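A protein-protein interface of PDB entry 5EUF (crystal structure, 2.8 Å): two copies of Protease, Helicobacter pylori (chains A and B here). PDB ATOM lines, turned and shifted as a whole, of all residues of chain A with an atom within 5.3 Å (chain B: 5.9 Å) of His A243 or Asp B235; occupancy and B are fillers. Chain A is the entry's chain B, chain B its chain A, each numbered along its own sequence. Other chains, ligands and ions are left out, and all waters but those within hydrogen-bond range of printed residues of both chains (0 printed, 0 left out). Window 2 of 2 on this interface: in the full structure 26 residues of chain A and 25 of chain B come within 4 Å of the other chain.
Among the printed residues, Asp or Glu carboxylates within 4 Å of a Lys or Arg side-chain nitrogen of the other chain: Arg A149 with Asp B235.
Among the printed residues, pairs that only touch across the chains: Arg A149 with Arg B238, Val A242 with Asp B235 and Met A145 with Asp B235.
No position is printed for both chains. Of the 8 pairs that touch across the chains among the printed residues, none has its exchanged pair printed and touching as well.
His A243 touches one residue of chain B. Of chain A, only Met A145, Arg A149, Val A241, Val A242 and His A243 come within 4 Å of Asp B235. Of the printed residues of chain A, Gly B236 touches Val A241 (3.2 Å). Printed residues of chain A within 4 Å of Arg B238: Arg A149 (3.5 Å). Of the printed residues of chain B, Val A241 touches Asp B235, Gly B236 and Ala B237. Printed residues of chain B within 4 Å of Arg A149: Asp B235 (3.96 Å) and Arg B238 (3.5 Å). Of the printed residues of chain A, Ala B237 touches Val A241 (2.9 Å). The nearest printed residue of chain A that does not touch Ala B237 is His A243 (5.8 Å).
The guanidinium group of Arg A149 lies within salt-bridge range of the side-chain carboxylate of Asp B235 (3.96 Å). N of His A243 sits at hydrogen-bond distance from O of Asp B235. The backbone NH (N) of Gly B236 sits close to the backbone carbonyl oxygen (O) of Val A241. The backbone carbonyl oxygen (O) of Ala B237 is in hydrogen-bond range of the backbone NH (N) of Val A241, 2.9 Å away. The backbone carbonyl oxygen of Val A241 lies close to the backbone carbonyl oxygen of Asp B235 (3.1 Å).
NE2 of Gln B234 is in hydrogen-bond range of O of Gly B236. The guanidinium group of Arg B238 lies within salt-bridge range of the side-chain carboxylate of Asp B235 (3.9 Å). N of Gly B236 is in hydrogen-bond range of O of Thr B410, at 3.0 Å. N of Val A242 lies within hydrogen-bond range of O of Phe A416 (2.7 Å). The backbone NH (N) of Lys A418 sits at hydrogen-bond distance from the backbone carbonyl oxygen (O) of Val A242.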
ATOM      1  N   MET A 145      -1.205 -17.507   0.516  1.00  0.00           N
ATOM      2  CA  MET A 145      -1.258 -18.016  -0.852  1.00  0.00           C
ATOM      3  C   MET A 145      -0.011 -17.619  -1.627  1.00  0.00           C
ATOM      4  O   MET A 145       0.545 -18.419  -2.378  1.00  0.00           O
ATOM      5  CB  MET A 145      -2.503 -17.500  -1.574  1.00  0.00           C
ATOM      6  CG  MET A 145      -2.718 -18.097  -2.955  1.00  0.00           C
ATOM      7  SD  MET A 145      -3.146 -19.997  -2.887  1.00  0.00           S
ATOM      8  CE  MET A 145      -3.564 -20.288  -4.773  1.00  0.00           C
ATOM      9  N   ARG A 149       2.415 -20.322  -3.310  1.00  0.00           N
ATOM     10  CA  ARG A 149       2.572 -20.293  -4.761  1.00  0.00           C
ATOM     11  C   ARG A 149       3.988 -19.902  -5.182  1.00  0.00           C
ATOM     12  O   ARG A 149       4.430 -20.247  -6.280  1.00  0.00           O
ATOM     13  CB  ARG A 149       1.559 -19.331  -5.393  1.00  0.00           C
ATOM     14  CG  ARG A 149       0.103 -19.772  -5.274  1.00  0.00           C
ATOM     15  CD  ARG A 149      -0.201 -21.013  -6.108  1.00  0.00           C
ATOM     16  NE  ARG A 149      -0.064 -20.773  -7.544  1.00  0.00           N
ATOM     17  CZ  ARG A 149       0.977 -21.168  -8.274  1.00  0.00           C
ATOM     18  NH1 ARG A 149       1.976 -21.828  -7.707  1.00  0.00           N
ATOM     19  NH2 ARG A 149       1.017 -20.906  -9.573  1.00  0.00           N
ATOM     20  N   VAL A 241       1.519 -15.671 -12.132  1.00  0.00           N
ATOM     21  CA  VAL A 241       0.522 -14.715 -11.675  1.00  0.00           C
ATOM     22  C   VAL A 241      -0.605 -15.453 -10.970  1.00  0.00           C
ATOM     23  O   VAL A 241      -1.110 -16.454 -11.476  1.00  0.00           O
ATOM     24  CB  VAL A 241      -0.045 -13.882 -12.839  1.00  0.00           C
ATOM     25  CG1 VAL A 241      -1.223 -13.044 -12.370  1.00  0.00           C
ATOM     26  CG2 VAL A 241       1.041 -13.001 -13.435  1.00  0.00           C
ATOM     27  N   VAL A 242      -0.988 -14.970  -9.792  1.00  0.00           N
ATOM     28  CA  VAL A 242      -2.074 -15.593  -9.049  1.00  0.00           C
ATOM     29  C   VAL A 242      -3.256 -14.643  -8.869  1.00  0.00           C
ATOM     30  O   VAL A 242      -3.184 -13.684  -8.102  1.00  0.00           O
ATOM     31  CB  VAL A 242      -1.602 -16.079  -7.669  1.00  0.00           C
ATOM     32  CG1 VAL A 242      -2.773 -16.638  -6.876  1.00  0.00           C
ATOM     33  CG2 VAL A 242      -0.510 -17.123  -7.827  1.00  0.00           C
ATOM     34  N   HIS A 243      -4.337 -14.915  -9.591  1.00  0.00           N
ATOM     35  CA  HIS A 243      -5.573 -14.164  -9.428  1.00  0.00           C
ATOM     36  C   HIS A 243      -6.439 -14.806  -8.349  1.00  0.00           C
ATOM     37  O   HIS A 243      -6.821 -15.971  -8.459  1.00  0.00           O
ATOM     38  CB  HIS A 243      -6.344 -14.083 -10.747  1.00  0.00           C
ATOM     39  CG  HIS A 243      -5.767 -13.108 -11.726  1.00  0.00           C
ATOM     40  ND1 HIS A 243      -6.045 -11.759 -11.682  1.00  0.00           N
ATOM     41  CD2 HIS A 243      -4.935 -13.287 -12.779  1.00  0.00           C
ATOM     42  CE1 HIS A 243      -5.404 -11.148 -12.662  1.00  0.00           C
ATOM     43  NE2 HIS A 243      -4.722 -12.052 -13.343  1.00  0.00           N
ATOM     44  N   LYS A 244      -6.737 -14.043  -7.301  1.00  0.00           N
ATOM     45  CA  LYS A 244      -7.572 -14.537  -6.214  1.00  0.00           C
ATOM     46  C   LYS A 244      -8.734 -13.584  -5.967  1.00  0.00           C
ATOM     47  O   LYS A 244      -8.579 -12.369  -6.073  1.00  0.00           O
ATOM     48  CB  LYS A 244      -6.747 -14.716  -4.939  1.00  0.00           C
ATOM     49  CG  LYS A 244      -7.277 -15.800  -4.016  1.00  0.00           C
ATOM     50  CD  LYS A 244      -7.277 -17.153  -4.717  1.00  0.00           C
ATOM     51  CE  LYS A 244      -7.951 -18.220  -3.872  1.00  0.00           C
ATOM     52  NZ  LYS A 244      -7.983 -19.536  -4.570  1.00  0.00           N
ATOM     53  N   ASP A 245      -9.898 -14.137  -5.643  1.00  0.00           N
ATOM     54  CA  ASP A 245     -11.095 -13.328  -5.439  1.00  0.00           C
ATOM     55  C   ASP A 245     -11.049 -12.563  -4.121  1.00  0.00           C
ATOM     56  O   ASP A 245     -11.423 -11.391  -4.061  1.00  0.00           O
ATOM     57  CB  ASP A 245     -12.348 -14.205  -5.488  1.00  0.00           C
ATOM     58  CG  ASP A 245     -12.637 -14.730  -6.879  1.00  0.00           C
ATOM     59  OD1 ASP A 245     -11.673 -14.969  -7.638  1.00  0.00           O
ATOM     60  OD2 ASP A 245     -13.828 -14.903  -7.214  1.00  0.00           O
ATOM     61  N   PHE A 416       3.110 -12.738  -8.679  1.00  0.00           N
ATOM     62  CA  PHE A 416       2.198 -11.608  -8.522  1.00  0.00           C
ATOM     63  C   PHE A 416       0.863 -12.045  -7.926  1.00  0.00           C
ATOM     64  O   PHE A 416       0.328 -13.097  -8.281  1.00  0.00           O
ATOM     65  CB  PHE A 416       1.957 -10.922  -9.869  1.00  0.00           C
ATOM     66  CG  PHE A 416       3.194 -10.332 -10.483  1.00  0.00           C
ATOM     67  CD1 PHE A 416       4.047  -9.539  -9.734  1.00  0.00           C
ATOM     68  CD2 PHE A 416       3.503 -10.572 -11.814  1.00  0.00           C
ATOM     69  CE1 PHE A 416       5.186  -8.994 -10.304  1.00  0.00           C
ATOM     70  CE2 PHE A 416       4.638 -10.031 -12.387  1.00  0.00           C
ATOM     71  CZ  PHE A 416       5.480  -9.241 -11.632  1.00  0.00           C
ATOM     72  N   LYS A 418      -2.999 -10.866  -7.624  1.00  0.00           N
ATOM     73  CA  LYS A 418      -3.998  -9.962  -8.181  1.00  0.00           C
ATOM     74  C   LYS A 418      -5.405 -10.515  -7.942  1.00  0.00           C
ATOM     75  O   LYS A 418      -5.550 -11.670  -7.543  1.00  0.00           O
ATOM     76  CB  LYS A 418      -3.745  -9.766  -9.679  1.00  0.00           C
ATOM     77  CG  LYS A 418      -2.401  -9.160 -10.016  1.00  0.00           C
ATOM     78  CD  LYS A 418      -2.234  -9.029 -11.519  1.00  0.00           C
ATOM     79  CE  LYS A 418      -0.957  -8.288 -11.865  1.00  0.00           C
ATOM     80  NZ  LYS A 418      -0.817  -8.079 -13.333  1.00  0.00           N
ATOM     81  N   PRO A 419      -6.450  -9.697  -8.153  1.00  0.00           N
ATOM     82  CA  PRO A 419      -6.467  -8.249  -8.394  1.00  0.00           C
ATOM     83  C   PRO A 419      -6.475  -7.463  -7.091  1.00  0.00           C
ATOM     84  O   PRO A 419      -7.399  -7.656  -6.301  1.00  0.00           O
ATOM     85  CB  PRO A 419      -7.775  -8.031  -9.171  1.00  0.00           C
ATOM     86  CG  PRO A 419      -8.250  -9.409  -9.559  1.00  0.00           C
ATOM     87  CD  PRO A 419      -7.752 -10.300  -8.477  1.00  0.00           C
ATOM     88  N   LYS B 233      -7.200 -25.043 -10.602  1.00  0.00           N
ATOM     89  CA  LYS B 233      -7.417 -24.217 -11.784  1.00  0.00           C
ATOM     90  C   LYS B 233      -6.328 -23.163 -11.883  1.00  0.00           C
ATOM     91  O   LYS B 233      -6.002 -22.509 -10.893  1.00  0.00           O
ATOM     92  CB  LYS B 233      -8.797 -23.558 -11.744  1.00  0.00           C
ATOM     93  N   GLN B 234      -5.747 -23.018 -13.070  1.00  0.00           N
ATOM     94  CA  GLN B 234      -4.674 -22.052 -13.263  1.00  0.00           C
ATOM     95  C   GLN B 234      -5.223 -20.643 -13.095  1.00  0.00           C
ATOM     96  O   GLN B 234      -6.277 -20.302 -13.633  1.00  0.00           O
ATOM     97  CB  GLN B 234      -4.012 -22.221 -14.630  1.00  0.00           C
ATOM     98  CG  GLN B 234      -2.780 -21.353 -14.816  1.00  0.00           C
ATOM     99  CD  GLN B 234      -1.905 -21.813 -15.963  1.00  0.00           C
ATOM    100  OE1 GLN B 234      -1.978 -22.965 -16.395  1.00  0.00           O
ATOM    101  NE2 GLN B 234      -1.064 -20.912 -16.462  1.00  0.00           N
ATOM    102  N   ASP B 235      -4.492 -19.834 -12.336  1.00  0.00           N
ATOM    103  CA  ASP B 235      -4.981 -18.547 -11.862  1.00  0.00           C
ATOM    104  C   ASP B 235      -4.212 -17.367 -12.448  1.00  0.00           C
ATOM    105  O   ASP B 235      -4.217 -16.276 -11.879  1.00  0.00           O
ATOM    106  CB  ASP B 235      -4.902 -18.510 -10.335  1.00  0.00           C
ATOM    107  CG  ASP B 235      -3.710 -19.294  -9.794  1.00  0.00           C
ATOM    108  OD1 ASP B 235      -2.773 -19.575 -10.573  1.00  0.00           O
ATOM    109  OD2 ASP B 235      -3.710 -19.629  -8.592  1.00  0.00           O
ATOM    110  N   GLY B 236      -3.556 -17.587 -13.582  1.00  0.00           N
ATOM    111  CA  GLY B 236      -2.749 -16.552 -14.204  1.00  0.00           C
ATOM    112  C   GLY B 236      -1.545 -17.125 -14.925  1.00  0.00           C
ATOM    113  O   GLY B 236      -1.170 -18.278 -14.706  1.00  0.00           O
ATOM    114  N   ALA B 237      -0.932 -16.313 -15.781  1.00  0.00           N
ATOM    115  CA  ALA B 237       0.166 -16.771 -16.627  1.00  0.00           C
ATOM    116  C   ALA B 237       1.368 -17.262 -15.825  1.00  0.00           C
ATOM    117  O   ALA B 237       1.769 -16.643 -14.839  1.00  0.00           O
ATOM    118  CB  ALA B 237       0.592 -15.658 -17.579  1.00  0.00           C
ATOM    119  N   ARG B 238       1.931 -18.385 -16.259  1.00  0.00           N
ATOM    120  CA  ARG B 238       3.170 -18.909 -15.695  1.00  0.00           C
ATOM    121  C   ARG B 238       4.245 -18.916 -16.773  1.00  0.00           C
ATOM    122  O   ARG B 238       3.982 -19.318 -17.907  1.00  0.00           O
ATOM    123  CB  ARG B 238       2.962 -20.319 -15.136  1.00  0.00           C
ATOM    124  CG  ARG B 238       1.855 -20.409 -14.100  1.00  0.00           C
ATOM    125  CD  ARG B 238       1.501 -21.847 -13.762  1.00  0.00           C
ATOM    126  NE  ARG B 238       0.328 -21.906 -12.891  1.00  0.00           N
ATOM    127  CZ  ARG B 238      -0.280 -23.029 -12.521  1.00  0.00           C
ATOM    128  NH1 ARG B 238       0.168 -24.202 -12.943  1.00  0.00           N
ATOM    129  NH2 ARG B 238      -1.341 -22.977 -11.728  1.00  0.00           N
ATOM    130  N   THR B 410      -4.377 -16.166 -18.871  1.00  0.00           N
ATOM    131  CA  THR B 410      -4.512 -16.619 -17.489  1.00  0.00           C
ATOM    132  C   THR B 410      -4.444 -18.142 -17.369  1.00  0.00           C
ATOM    133  O   THR B 410      -4.337 -18.683 -16.266  1.00  0.00           O
ATOM    134  CB  THR B 410      -5.830 -16.127 -16.861  1.00  0.00           C
ATOM    135  OG1 THR B 410      -6.929 -16.473 -17.715  1.00  0.00           O
ATOM    136  CG2 THR B 410      -5.796 -14.620 -16.667  1.00  0.00           C
